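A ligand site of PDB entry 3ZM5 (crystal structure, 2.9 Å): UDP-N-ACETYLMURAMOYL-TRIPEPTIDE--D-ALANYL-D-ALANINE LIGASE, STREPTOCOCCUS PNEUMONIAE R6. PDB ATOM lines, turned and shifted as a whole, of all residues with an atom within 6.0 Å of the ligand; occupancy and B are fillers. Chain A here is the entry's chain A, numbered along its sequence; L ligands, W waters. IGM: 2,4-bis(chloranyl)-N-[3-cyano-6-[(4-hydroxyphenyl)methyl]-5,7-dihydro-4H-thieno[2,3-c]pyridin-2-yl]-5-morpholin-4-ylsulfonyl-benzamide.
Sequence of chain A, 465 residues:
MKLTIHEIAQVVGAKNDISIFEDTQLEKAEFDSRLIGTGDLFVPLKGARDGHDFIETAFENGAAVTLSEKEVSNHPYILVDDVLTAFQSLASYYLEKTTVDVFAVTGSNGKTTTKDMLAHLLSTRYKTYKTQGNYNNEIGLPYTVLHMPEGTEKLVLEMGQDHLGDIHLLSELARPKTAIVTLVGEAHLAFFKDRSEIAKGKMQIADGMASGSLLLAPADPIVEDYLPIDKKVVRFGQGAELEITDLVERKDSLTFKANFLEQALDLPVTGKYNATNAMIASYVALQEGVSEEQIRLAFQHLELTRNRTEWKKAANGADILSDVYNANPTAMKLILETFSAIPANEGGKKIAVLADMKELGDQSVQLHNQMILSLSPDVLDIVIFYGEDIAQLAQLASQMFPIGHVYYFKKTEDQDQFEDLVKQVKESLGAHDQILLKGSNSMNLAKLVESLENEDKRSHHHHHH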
ATOM      1  N   PHE A  31      14.474 -32.557  -5.253  1.00  0.00           N
ATOM      2  CA  PHE A  31      13.507 -31.463  -5.144  1.00  0.00           C
ATOM      3  C   PHE A  31      13.403 -30.588  -6.398  1.00  0.00           C
ATOM      4  O   PHE A  31      12.471 -29.825  -6.534  1.00  0.00           O
ATOM      5  CB  PHE A  31      13.759 -30.604  -3.907  1.00  0.00           C
ATOM      6  CG  PHE A  31      15.147 -30.018  -3.841  1.00  0.00           C
ATOM      7  CD1 PHE A  31      15.520 -28.967  -4.684  1.00  0.00           C
ATOM      8  CD2 PHE A  31      16.067 -30.483  -2.905  1.00  0.00           C
ATOM      9  CE1 PHE A  31      16.784 -28.413  -4.596  1.00  0.00           C
ATOM     10  CE2 PHE A  31      17.332 -29.935  -2.809  1.00  0.00           C
ATOM     11  CZ  PHE A  31      17.694 -28.898  -3.661  1.00  0.00           C
ATOM     12  N   ASP A  32      14.375 -30.710  -7.299  1.00  0.00           N
ATOM     13  CA  ASP A  32      14.420 -29.904  -8.527  1.00  0.00           C
ATOM     14  C   ASP A  32      13.882 -30.743  -9.680  1.00  0.00           C
ATOM     15  O   ASP A  32      14.589 -31.575 -10.229  1.00  0.00           O
ATOM     16  CB  ASP A  32      15.866 -29.422  -8.768  1.00  0.00           C
ATOM     17  CG  ASP A  32      16.047 -28.703 -10.130  1.00  0.00           C
ATOM     18  OD1 ASP A  32      15.079 -28.150 -10.673  1.00  0.00           O
ATOM     19  OD2 ASP A  32      17.185 -28.688 -10.660  1.00  0.00           O
ATOM     20  N   SER A  33      12.622 -30.521 -10.054  1.00  0.00           N
ATOM     21  CA  SER A  33      11.926 -31.387 -11.039  1.00  0.00           C
ATOM     22  C   SER A  33      12.782 -31.820 -12.244  1.00  0.00           C
ATOM     23  O   SER A  33      12.711 -32.958 -12.692  1.00  0.00           O
ATOM     24  CB  SER A  33      10.615 -30.734 -11.517  1.00  0.00           C
ATOM     25  OG  SER A  33      10.721 -29.310 -11.539  1.00  0.00           O
ATOM     26  N   ARG A  34      13.580 -30.898 -12.750  1.00  0.00           N
ATOM     27  CA  ARG A  34      14.406 -31.161 -13.903  1.00  0.00           C
ATOM     28  C   ARG A  34      15.354 -32.356 -13.733  1.00  0.00           C
ATOM     29  O   ARG A  34      15.926 -32.844 -14.709  1.00  0.00           O
ATOM     30  CB  ARG A  34      15.200 -29.903 -14.253  1.00  0.00           C
ATOM     31  CG  ARG A  34      14.363 -28.717 -14.658  1.00  0.00           C
ATOM     32  CD  ARG A  34      15.212 -27.473 -14.778  1.00  0.00           C
ATOM     33  NE  ARG A  34      15.763 -27.093 -13.474  1.00  0.00           N
ATOM     34  CZ  ARG A  34      16.505 -26.009 -13.270  1.00  0.00           C
ATOM     35  NH1 ARG A  34      16.783 -25.194 -14.268  1.00  0.00           N
ATOM     36  NH2 ARG A  34      16.972 -25.744 -12.060  1.00  0.00           N
ATOM     37  N   LEU A  45       9.628 -28.546  -1.871  1.00  0.00           N
ATOM     38  CA  LEU A  45       9.907 -27.600  -0.811  1.00  0.00           C
ATOM     39  C   LEU A  45       9.400 -26.181  -1.088  1.00  0.00           C
ATOM     40  O   LEU A  45       9.079 -25.830  -2.238  1.00  0.00           O
ATOM     41  CB  LEU A  45      11.412 -27.572  -0.532  1.00  0.00           C
ATOM     42  CG  LEU A  45      12.054 -28.887  -0.065  1.00  0.00           C
ATOM     43  CD1 LEU A  45      13.581 -28.770  -0.073  1.00  0.00           C
ATOM     44  CD2 LEU A  45      11.556 -29.289   1.314  1.00  0.00           C
ATOM     45  N   LYS A  46       9.345 -25.357  -0.039  1.00  0.00           N
ATOM     46  CA  LYS A  46       9.077 -23.914  -0.163  1.00  0.00           C
ATOM     47  C   LYS A  46      10.228 -23.154  -0.828  1.00  0.00           C
ATOM     48  O   LYS A  46      11.120 -22.636  -0.162  1.00  0.00           O
ATOM     49  CB  LYS A  46       8.766 -23.295   1.215  1.00  0.00           C
ATOM     50  CG  LYS A  46       7.634 -23.998   1.943  1.00  0.00           C
ATOM     51  CD  LYS A  46       7.444 -23.509   3.369  1.00  0.00           C
ATOM     52  CE  LYS A  46       6.411 -24.394   4.050  1.00  0.00           C
ATOM     53  NZ  LYS A  46       6.693 -24.571   5.506  1.00  0.00           N
ATOM     54  N   GLY A  47      10.207 -23.091  -2.159  1.00  0.00           N
ATOM     55  CA  GLY A  47      11.194 -22.306  -2.893  1.00  0.00           C
ATOM     56  C   GLY A  47      10.586 -21.011  -3.367  1.00  0.00           C
ATOM     57  O   GLY A  47       9.637 -20.494  -2.758  1.00  0.00           O
ATOM     58  N   ALA A  48      11.133 -20.465  -4.452  1.00  0.00           N
ATOM     59  CA  ALA A  48      10.541 -19.293  -5.129  1.00  0.00           C
ATOM     60  C   ALA A  48       9.039 -19.476  -5.360  1.00  0.00           C
ATOM     61  O   ALA A  48       8.236 -18.543  -5.206  1.00  0.00           O
ATOM     62  CB  ALA A  48      11.256 -19.026  -6.455  1.00  0.00           C
ATOM     63  N   ARG A  49       8.678 -20.690  -5.742  1.00  0.00           N
ATOM     64  CA  ARG A  49       7.313 -21.148  -5.707  1.00  0.00           C
ATOM     65  C   ARG A  49       7.278 -22.403  -4.866  1.00  0.00           C
ATOM     66  O   ARG A  49       8.304 -23.030  -4.634  1.00  0.00           O
ATOM     67  CB  ARG A  49       6.793 -21.411  -7.106  1.00  0.00           C
ATOM     68  CG  ARG A  49       6.327 -20.134  -7.790  1.00  0.00           C
ATOM     69  CD  ARG A  49       5.637 -20.455  -9.092  1.00  0.00           C
ATOM     70  NE  ARG A  49       4.402 -19.682  -9.198  1.00  0.00           N
ATOM     71  CZ  ARG A  49       3.208 -20.161  -8.857  1.00  0.00           C
ATOM     72  NH1 ARG A  49       3.094 -21.406  -8.393  1.00  0.00           N
ATOM     73  NH2 ARG A  49       2.123 -19.403  -8.984  1.00  0.00           N
ATOM     74  N   ASP A  50       6.116 -22.770  -4.362  1.00  0.00           N
ATOM     75  CA  ASP A  50       6.026 -23.972  -3.586  1.00  0.00           C
ATOM     76  C   ASP A  50       6.313 -25.175  -4.448  1.00  0.00           C
ATOM     77  O   ASP A  50       5.903 -25.241  -5.598  1.00  0.00           O
ATOM     78  CB  ASP A  50       4.639 -24.154  -3.001  1.00  0.00           C
ATOM     79  CG  ASP A  50       4.475 -25.510  -2.361  1.00  0.00           C
ATOM     80  OD1 ASP A  50       5.197 -25.784  -1.368  1.00  0.00           O
ATOM     81  OD2 ASP A  50       3.675 -26.311  -2.874  1.00  0.00           O
ATOM     82  N   GLY A  51       6.998 -26.160  -3.874  1.00  0.00           N
ATOM     83  CA  GLY A  51       7.279 -27.391  -4.569  1.00  0.00           C
ATOM     84  C   GLY A  51       6.056 -28.014  -5.185  1.00  0.00           C
ATOM     85  O   GLY A  51       6.083 -28.414  -6.334  1.00  0.00           O
ATOM     86  N   PHE A  54       4.914 -28.371  -8.753  1.00  0.00           N
ATOM     87  CA  PHE A  54       5.640 -29.172  -9.717  1.00  0.00           C
ATOM     88  C   PHE A  54       5.572 -30.687  -9.431  1.00  0.00           C
ATOM     89  O   PHE A  54       6.366 -31.460  -9.952  1.00  0.00           O
ATOM     90  CB  PHE A  54       7.085 -28.674  -9.823  1.00  0.00           C
ATOM     91  CG  PHE A  54       7.202 -27.181  -9.860  1.00  0.00           C
ATOM     92  CD1 PHE A  54       7.048 -26.481 -11.058  1.00  0.00           C
ATOM     93  CD2 PHE A  54       7.456 -26.458  -8.696  1.00  0.00           C
ATOM     94  CE1 PHE A  54       7.136 -25.096 -11.106  1.00  0.00           C
ATOM     95  CE2 PHE A  54       7.553 -25.083  -8.740  1.00  0.00           C
ATOM     96  CZ  PHE A  54       7.395 -24.396  -9.935  1.00  0.00           C
ATOM     97  N   THR A  57       4.524 -31.969 -12.698  1.00  0.00           N
ATOM     98  CA  THR A  57       5.609 -32.103 -13.649  1.00  0.00           C
ATOM     99  C   THR A  57       6.575 -33.213 -13.297  1.00  0.00           C
ATOM    100  O   THR A  57       7.168 -33.822 -14.190  1.00  0.00           O
ATOM    101  CB  THR A  57       6.402 -30.777 -13.814  1.00  0.00           C
ATOM    102  OG1 THR A  57       5.814 -29.996 -14.873  1.00  0.00           O
ATOM    103  CG2 THR A  57       7.884 -31.041 -14.139  1.00  0.00           C
ATOM    104  N   ASN A 134      27.823 -26.371  -2.586  1.00  0.00           N
ATOM    105  CA  ASN A 134      27.542 -25.712  -1.309  1.00  0.00           C
ATOM    106  C   ASN A 134      26.259 -26.175  -0.569  1.00  0.00           C
ATOM    107  O   ASN A 134      25.606 -25.398   0.119  1.00  0.00           O
ATOM    108  CB  ASN A 134      27.549 -24.204  -1.466  1.00  0.00           C
ATOM    109  CG  ASN A 134      26.300 -23.687  -2.089  1.00  0.00           C
ATOM    110  OD1 ASN A 134      25.426 -24.474  -2.468  1.00  0.00           O
ATOM    111  ND2 ASN A 134      26.194 -22.364  -2.212  1.00  0.00           N
ATOM    112  N   TYR A 135      25.924 -27.452  -0.740  1.00  0.00           N
ATOM    113  CA  TYR A 135      24.797 -28.081  -0.095  1.00  0.00           C
ATOM    114  C   TYR A 135      25.140 -28.438   1.357  1.00  0.00           C
ATOM    115  O   TYR A 135      25.356 -29.618   1.703  1.00  0.00           O
ATOM    116  CB  TYR A 135      24.407 -29.336  -0.876  1.00  0.00           C
ATOM    117  CG  TYR A 135      23.576 -29.039  -2.096  1.00  0.00           C
ATOM    118  CD1 TYR A 135      23.807 -27.901  -2.866  1.00  0.00           C
ATOM    119  CD2 TYR A 135      22.536 -29.887  -2.468  1.00  0.00           C
ATOM    120  CE1 TYR A 135      23.045 -27.630  -3.967  1.00  0.00           C
ATOM    121  CE2 TYR A 135      21.762 -29.625  -3.585  1.00  0.00           C
ATOM    122  CZ  TYR A 135      22.024 -28.497  -4.330  1.00  0.00           C
ATOM    123  OH  TYR A 135      21.264 -28.207  -5.443  1.00  0.00           O
ATOM    124  N   ASN A 136      25.136 -27.424   2.213  1.00  0.00           N
ATOM    125  CA  ASN A 136      25.596 -27.576   3.596  1.00  0.00           C
ATOM    126  C   ASN A 136      24.594 -27.184   4.658  1.00  0.00           C
ATOM    127  O   ASN A 136      24.984 -27.040   5.793  1.00  0.00           O
ATOM    128  CB  ASN A 136      26.860 -26.726   3.809  1.00  0.00           C
ATOM    129  CG  ASN A 136      26.574 -25.224   3.743  1.00  0.00           C
ATOM    130  OD1 ASN A 136      25.471 -24.754   4.070  1.00  0.00           O
ATOM    131  ND2 ASN A 136      27.571 -24.461   3.352  1.00  0.00           N
ATOM    132  N   ASN A 137      23.328 -26.999   4.307  1.00  0.00           N
ATOM    133  CA  ASN A 137      22.366 -26.500   5.304  1.00  0.00           C
ATOM    134  C   ASN A 137      21.232 -27.487   5.592  1.00  0.00           C
ATOM    135  O   ASN A 137      21.393 -28.670   5.373  1.00  0.00           O
ATOM    136  CB  ASN A 137      21.786 -25.174   4.859  1.00  0.00           C
ATOM    137  CG  ASN A 137      21.022 -25.300   3.573  1.00  0.00           C
ATOM    138  OD1 ASN A 137      21.455 -26.022   2.673  1.00  0.00           O
ATOM    139  ND2 ASN A 137      19.888 -24.639   3.483  1.00  0.00           N
ATOM    140  N   ILE A 139      18.476 -27.906   4.074  1.00  0.00           N
ATOM    141  CA  ILE A 139      18.125 -28.582   2.835  1.00  0.00           C
ATOM    142  C   ILE A 139      19.336 -29.390   2.347  1.00  0.00           C
ATOM    143  O   ILE A 139      19.201 -30.576   2.011  1.00  0.00           O
ATOM    144  CB  ILE A 139      17.702 -27.590   1.753  1.00  0.00           C
ATOM    145  CG1 ILE A 139      16.345 -26.966   2.106  1.00  0.00           C
ATOM    146  CG2 ILE A 139      17.589 -28.303   0.425  1.00  0.00           C
ATOM    147  CD1 ILE A 139      16.301 -25.459   1.968  1.00  0.00           C
ATOM    148  N   GLY A 140      20.519 -28.766   2.349  1.00  0.00           N
ATOM    149  CA  GLY A 140      21.723 -29.311   1.728  1.00  0.00           C
ATOM    150  C   GLY A 140      22.246 -30.624   2.290  1.00  0.00           C
ATOM    151  O   GLY A 140      22.654 -31.524   1.553  1.00  0.00           O
ATOM    152  N   ASN A 326      24.691 -22.505  -7.866  1.00  0.00           N
ATOM    153  CA  ASN A 326      23.255 -22.764  -7.938  1.00  0.00           C
ATOM    154  C   ASN A 326      22.507 -21.860  -8.871  1.00  0.00           C
ATOM    155  O   ASN A 326      22.142 -20.751  -8.511  1.00  0.00           O
ATOM    156  CB  ASN A 326      22.612 -22.750  -6.546  1.00  0.00           C
ATOM    157  CG  ASN A 326      23.051 -23.918  -5.693  1.00  0.00           C
ATOM    158  OD1 ASN A 326      22.779 -25.087  -6.007  1.00  0.00           O
ATOM    159  ND2 ASN A 326      23.759 -23.612  -4.615  1.00  0.00           N
ATOM    160  N   ASN A 328      19.248 -21.398 -10.283  1.00  0.00           N
ATOM    161  CA  ASN A 328      17.844 -21.756 -10.071  1.00  0.00           C
ATOM    162  C   ASN A 328      17.144 -20.701  -9.263  1.00  0.00           C
ATOM    163  O   ASN A 328      17.785 -19.988  -8.503  1.00  0.00           O
ATOM    164  CB  ASN A 328      17.660 -23.171  -9.445  1.00  0.00           C
ATOM    165  CG  ASN A 328      17.780 -23.182  -7.932  1.00  0.00           C
ATOM    166  OD1 ASN A 328      17.623 -22.174  -7.268  1.00  0.00           O
ATOM    167  ND2 ASN A 328      18.031 -24.351  -7.372  1.00  0.00           N
ATOM    168  N   PRO A 329      15.824 -20.582  -9.416  1.00  0.00           N
ATOM    169  CA  PRO A 329      15.117 -19.441  -8.855  1.00  0.00           C
ATOM    170  C   PRO A 329      15.184 -19.364  -7.331  1.00  0.00           C
ATOM    171  O   PRO A 329      15.553 -18.312  -6.806  1.00  0.00           O
ATOM    172  CB  PRO A 329      13.691 -19.605  -9.369  1.00  0.00           C
ATOM    173  CG  PRO A 329      13.589 -21.026  -9.767  1.00  0.00           C
ATOM    174  CD  PRO A 329      14.941 -21.453 -10.213  1.00  0.00           C
ATOM    175  N   THR A 330      14.871 -20.433  -6.623  1.00  0.00           N
ATOM    176  CA  THR A 330      14.943 -20.366  -5.157  1.00  0.00           C
ATOM    177  C   THR A 330      16.279 -19.794  -4.683  1.00  0.00           C
ATOM    178  O   THR A 330      16.337 -19.059  -3.715  1.00  0.00           O
ATOM    179  CB  THR A 330      14.703 -21.712  -4.486  1.00  0.00           C
ATOM    180  OG1 THR A 330      13.507 -22.282  -4.993  1.00  0.00           O
ATOM    181  CG2 THR A 330      14.554 -21.530  -2.990  1.00  0.00           C
ATOM    182  N   ALA A 331      17.352 -20.133  -5.395  1.00  0.00           N
ATOM    183  CA  ALA A 331      18.683 -19.608  -5.091  1.00  0.00           C
ATOM    184  C   ALA A 331      18.790 -18.123  -5.442  1.00  0.00           C
ATOM    185  O   ALA A 331      19.487 -17.364  -4.782  1.00  0.00           O
ATOM    186  CB  ALA A 331      19.763 -20.422  -5.798  1.00  0.00           C
ATOM    187  N   LEU A 334      16.842 -16.606  -2.501  1.00  0.00           N
ATOM    188  CA  LEU A 334      17.504 -16.710  -1.215  1.00  0.00           C
ATOM    189  C   LEU A 334      18.604 -15.675  -1.041  1.00  0.00           C
ATOM    190  O   LEU A 334      18.793 -15.146   0.043  1.00  0.00           O
ATOM    191  CB  LEU A 334      18.060 -18.115  -0.998  1.00  0.00           C
ATOM    192  CG  LEU A 334      17.013 -19.211  -0.702  1.00  0.00           C
ATOM    193  CD1 LEU A 334      17.692 -20.554  -0.485  1.00  0.00           C
ATOM    194  CD2 LEU A 334      16.155 -18.826   0.494  1.00  0.00           C
ATOM    195  N   GLU A 359      17.252 -22.626 -18.419  1.00  0.00           N
ATOM    196  CA  GLU A 359      16.603 -23.915 -18.238  1.00  0.00           C
ATOM    197  C   GLU A 359      15.336 -23.885 -17.420  1.00  0.00           C
ATOM    198  O   GLU A 359      15.123 -24.763 -16.577  1.00  0.00           O
ATOM    199  CB  GLU A 359      17.547 -24.946 -17.627  1.00  0.00           C
ATOM    200  CG  GLU A 359      18.564 -25.545 -18.592  1.00  0.00           C
ATOM    201  CD  GLU A 359      19.915 -24.880 -18.450  1.00  0.00           C
ATOM    202  OE1 GLU A 359      20.204 -24.373 -17.336  1.00  0.00           O
ATOM    203  OE2 GLU A 359      20.669 -24.861 -19.438  1.00  0.00           O
ATOM    204  N   LEU A 360      14.487 -22.896 -17.667  1.00  0.00           N
ATOM    205  CA  LEU A 360      13.172 -22.887 -17.030  1.00  0.00           C
ATOM    206  C   LEU A 360      12.020 -23.209 -18.024  1.00  0.00           C
ATOM    207  O   LEU A 360      10.832 -23.030 -17.707  1.00  0.00           O
ATOM    208  CB  LEU A 360      12.954 -21.568 -16.282  1.00  0.00           C
ATOM    209  CG  LEU A 360      14.018 -21.132 -15.279  1.00  0.00           C
ATOM    210  CD1 LEU A 360      13.620 -19.854 -14.544  1.00  0.00           C
ATOM    211  CD2 LEU A 360      14.286 -22.246 -14.284  1.00  0.00           C
ATOM    212  N   GLY A 361      12.384 -23.687 -19.221  1.00  0.00           N
ATOM    213  CA  GLY A 361      11.419 -24.019 -20.264  1.00  0.00           C
ATOM    214  C   GLY A 361      10.224 -23.076 -20.291  1.00  0.00           C
ATOM    215  O   GLY A 361      10.404 -21.870 -20.407  1.00  0.00           O
ATOM    216  N   ASP A 362       9.028 -23.635 -20.156  1.00  0.00           N
ATOM    217  CA  ASP A 362       7.767 -22.899 -20.308  1.00  0.00           C
ATOM    218  C   ASP A 362       7.301 -22.235 -18.998  1.00  0.00           C
ATOM    219  O   ASP A 362       6.099 -22.141 -18.729  1.00  0.00           O
ATOM    220  CB  ASP A 362       6.670 -23.824 -20.826  1.00  0.00           C
ATOM    221  CG  ASP A 362       6.425 -25.034 -19.919  1.00  0.00           C
ATOM    222  OD1 ASP A 362       7.391 -25.506 -19.256  1.00  0.00           O
ATOM    223  OD2 ASP A 362       5.278 -25.519 -19.876  1.00  0.00           O
ATOM    224  N   GLN A 363       8.249 -21.783 -18.202  1.00  0.00           N
ATOM    225  CA  GLN A 363       7.941 -21.190 -16.919  1.00  0.00           C
ATOM    226  C   GLN A 363       8.898 -20.010 -16.655  1.00  0.00           C
ATOM    227  O   GLN A 363       8.748 -19.256 -15.691  1.00  0.00           O
ATOM    228  CB  GLN A 363       8.064 -22.260 -15.845  1.00  0.00           C
ATOM    229  CG  GLN A 363       7.150 -22.056 -14.647  1.00  0.00           C
ATOM    230  CD  GLN A 363       5.696 -22.273 -14.971  1.00  0.00           C
ATOM    231  OE1 GLN A 363       5.346 -23.178 -15.741  1.00  0.00           O
ATOM    232  NE2 GLN A 363       4.834 -21.472 -14.369  1.00  0.00           N
ATOM    233  N   SER A 364       9.896 -19.870 -17.519  1.00  0.00           N
ATOM    234  CA  SER A 364      10.915 -18.862 -17.340  1.00  0.00           C
ATOM    235  C   SER A 364      10.292 -17.559 -16.875  1.00  0.00           C
ATOM    236  O   SER A 364      10.534 -17.125 -15.743  1.00  0.00           O
ATOM    237  CB  SER A 364      11.680 -18.625 -18.632  1.00  0.00           C
ATOM    238  OG  SER A 364      12.808 -17.817 -18.390  1.00  0.00           O
ATOM    239  N   LEU A 367       8.550 -17.343 -13.673  1.00  0.00           N
ATOM    240  CA  LEU A 367       9.493 -17.519 -12.582  1.00  0.00           C
ATOM    241  C   LEU A 367      10.362 -16.307 -12.332  1.00  0.00           C
ATOM    242  O   LEU A 367      10.704 -16.008 -11.189  1.00  0.00           O
ATOM    243  CB  LEU A 367      10.375 -18.723 -12.818  1.00  0.00           C
ATOM    244  CG  LEU A 367       9.659 -20.064 -12.652  1.00  0.00           C
ATOM    245  CD1 LEU A 367      10.554 -21.206 -13.144  1.00  0.00           C
ATOM    246  CD2 LEU A 367       9.233 -20.276 -11.197  1.00  0.00           C
HETATM  247  O25 IGM L   1      19.877 -24.017  -4.479  1.00  0.00           O
HETATM  248  S21 IGM L   1      19.262 -23.845  -3.202  1.00  0.00           S
HETATM  249  O24 IGM L   1      19.244 -22.429  -2.925  1.00  0.00           O
HETATM  250  N23 IGM L   1      19.992 -24.561  -2.056  1.00  0.00           N
HETATM  251  C27 IGM L   1      20.317 -25.974  -2.343  1.00  0.00           C
HETATM  252  C29 IGM L   1      21.005 -26.618  -1.151  1.00  0.00           C
HETATM  253  O31 IGM L   1      21.142 -25.691  -0.070  1.00  0.00           O
HETATM  254  C30 IGM L   1      21.837 -24.478  -0.387  1.00  0.00           C
HETATM  255  C28 IGM L   1      21.159 -23.789  -1.573  1.00  0.00           C
HETATM  256  C18 IGM L   1      17.685 -24.402  -3.317  1.00  0.00           C
HETATM  257  C22 IGM L   1      16.979 -24.681  -2.163  1.00  0.00           C
HETATM  258 CL2  IGM L   1      17.759 -24.462  -0.551  1.00  0.00          CL
HETATM  259  C19 IGM L   1      15.673 -25.132  -2.257  1.00  0.00           C
HETATM  260  C17 IGM L   1      15.094 -25.294  -3.500  1.00  0.00           C
HETATM  261 CL1  IGM L   1      13.427 -25.876  -3.580  1.00  0.00          CL
HETATM  262  C16 IGM L   1      17.113 -24.562  -4.571  1.00  0.00           C
HETATM  263  C14 IGM L   1      15.807 -25.014  -4.641  1.00  0.00           C
HETATM  264  C13 IGM L   1      15.218 -25.182  -5.998  1.00  0.00           C
HETATM  265  O15 IGM L   1      15.866 -25.845  -6.777  1.00  0.00           O
HETATM  266  N10 IGM L   1      14.054 -24.608  -6.319  1.00  0.00           N
HETATM  267  C5  IGM L   1      13.554 -24.790  -7.577  1.00  0.00           C
HETATM  268  C2  IGM L   1      12.313 -24.202  -8.125  1.00  0.00           C
HETATM  269  C6  IGM L   1      11.454 -23.372  -7.367  1.00  0.00           C
HETATM  270  N11 IGM L   1      10.694 -22.735  -6.775  1.00  0.00           N
HETATM  271  S7  IGM L   1      14.305 -25.746  -8.794  1.00  0.00           S
HETATM  272  C3  IGM L   1      13.097 -25.463 -10.015  1.00  0.00           C
HETATM  273  C1  IGM L   1      12.015 -24.585  -9.546  1.00  0.00           C
HETATM  274  C8  IGM L   1      13.204 -26.089 -11.364  1.00  0.00           C
HETATM  275  N12 IGM L   1      12.284 -25.404 -12.253  1.00  0.00           N
HETATM  276  C9  IGM L   1      11.379 -24.292 -11.906  1.00  0.00           C
HETATM  277  C4  IGM L   1      10.884 -24.264 -10.466  1.00  0.00           C
HETATM  278  C32 IGM L   1      12.341 -25.803 -13.643  1.00  0.00           C
HETATM  279  C33 IGM L   1      10.985 -26.000 -14.279  1.00  0.00           C
HETATM  280  C38 IGM L   1      10.701 -25.334 -15.469  1.00  0.00           C
HETATM  281  C37 IGM L   1       9.469 -25.505 -16.093  1.00  0.00           C
HETATM  282  C36 IGM L   1       8.532 -26.374 -15.552  1.00  0.00           C
HETATM  283  O39 IGM L   1       7.315 -26.542 -16.176  1.00  0.00           O
HETATM  284  C35 IGM L   1       8.841 -27.046 -14.382  1.00  0.00           C
HETATM  285  C34 IGM L   1      10.056 -26.873 -13.742  1.00  0.00           C
HETATM  286  O   HOH W   1      10.141 -25.893  -5.533  1.00  0.00           O
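The side-chain carboxylate (OD1) of Asp 32 sits close to a sulfur (S7) of the ligand (3.1 Å).
Phe 31 touches the ligand (CE1 to O15, 3.5 Å).
OG of Ser 33 touches C34 of the ligand, 3.4 Å away.
NE of Arg 34 touches C8 of the ligand, at 3.5 Å.
Gly 47 touches the ligand.
Phe 54 touches the ligand.
OG1 of Thr 57 touches O39 of the ligand, at 3.99 Å.
Asn 134 touches the ligand.
Tyr 135 touches the ligand (CD1 to C29, 3.5 Å).
CD1 of Ile 139 touches CL2 of the ligand (3.1 Å).
Gly 140 touches the ligand.
Pro 329 touches the ligand (CG to C2, 3.8 Å).
Ala 331 touches the ligand (CB to O24, 3.5 Å).
Leu 334 touches the ligand.
O of Leu 360 touches C38 of the ligand (3.2 Å).
Gln 363 touches the ligand (CB to C37, 3.5 Å).
CD1 of Leu 367 touches C9 of the ligand, at 3.4 Å.
Hydrophobic or aromatic side chains that line the ligand: Phe 31, Ala 48, Phe 54, Tyr 135, Ile 139, Pro 329, Ala 331, Leu 334 and Leu 367.
The side-chain carboxylate (OD1) of Asp 362 lies within hydrogen-bond range of an oxygen (O39) of the ligand, 3.3 Å away.
A nitrogen (N10) of the ligand sits at hydrogen-bond distance from the side-chain hydroxyl of Thr 330.
The side-chain amide nitrogen of Asn 328 sits at hydrogen-bond distance from an oxygen (O15) of the ligand (2.7 Å).
A nitrogen (N11) of the ligand is in hydrogen-bond range of the backbone NH of Arg 49 (3.1 Å).
O31 of the ligand lies close to OD1 of Asn 137 (2.8 Å).
OD1 of Asn 326 lies close to O25 of the ligand, at 3.4 Å.
A nitrogen (N11) of the ligand sits at hydrogen-bond distance from the backbone NH (N) of Ala 48 (3.3 Å).
Water W1 bridges N11 of the ligand (3.4 Å) and O of Leu 45 (3.5 Å).
OD1 of Asn 328 lies within hydrogen-bond range of N of Thr 330.
The side-chain amide nitrogen (ND2) of Asn 326 is in hydrogen-bond range of the side-chain amide oxygen (OD1) of Asn 134.
The backbone NH of Gly 140 sits at hydrogen-bond distance from the side-chain amide oxygen of Asn 137 (2.9 Å).
The backbone NH of Ala 48 sits at hydrogen-bond distance from the side-chain hydroxyl of Thr 330, at 3.0 Å.
OD1 of Asp 32 lies within salt-bridge range of NE of Arg 34.
The side-chain amide oxygen of Asn 328 is in hydrogen-bond range of the backbone NH of Ala 331.
The guanidinium group (NH1) of Arg 34 lies within hydrogen-bond range of the backbone carbonyl oxygen (O) of Glu 359, at 2.9 Å.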
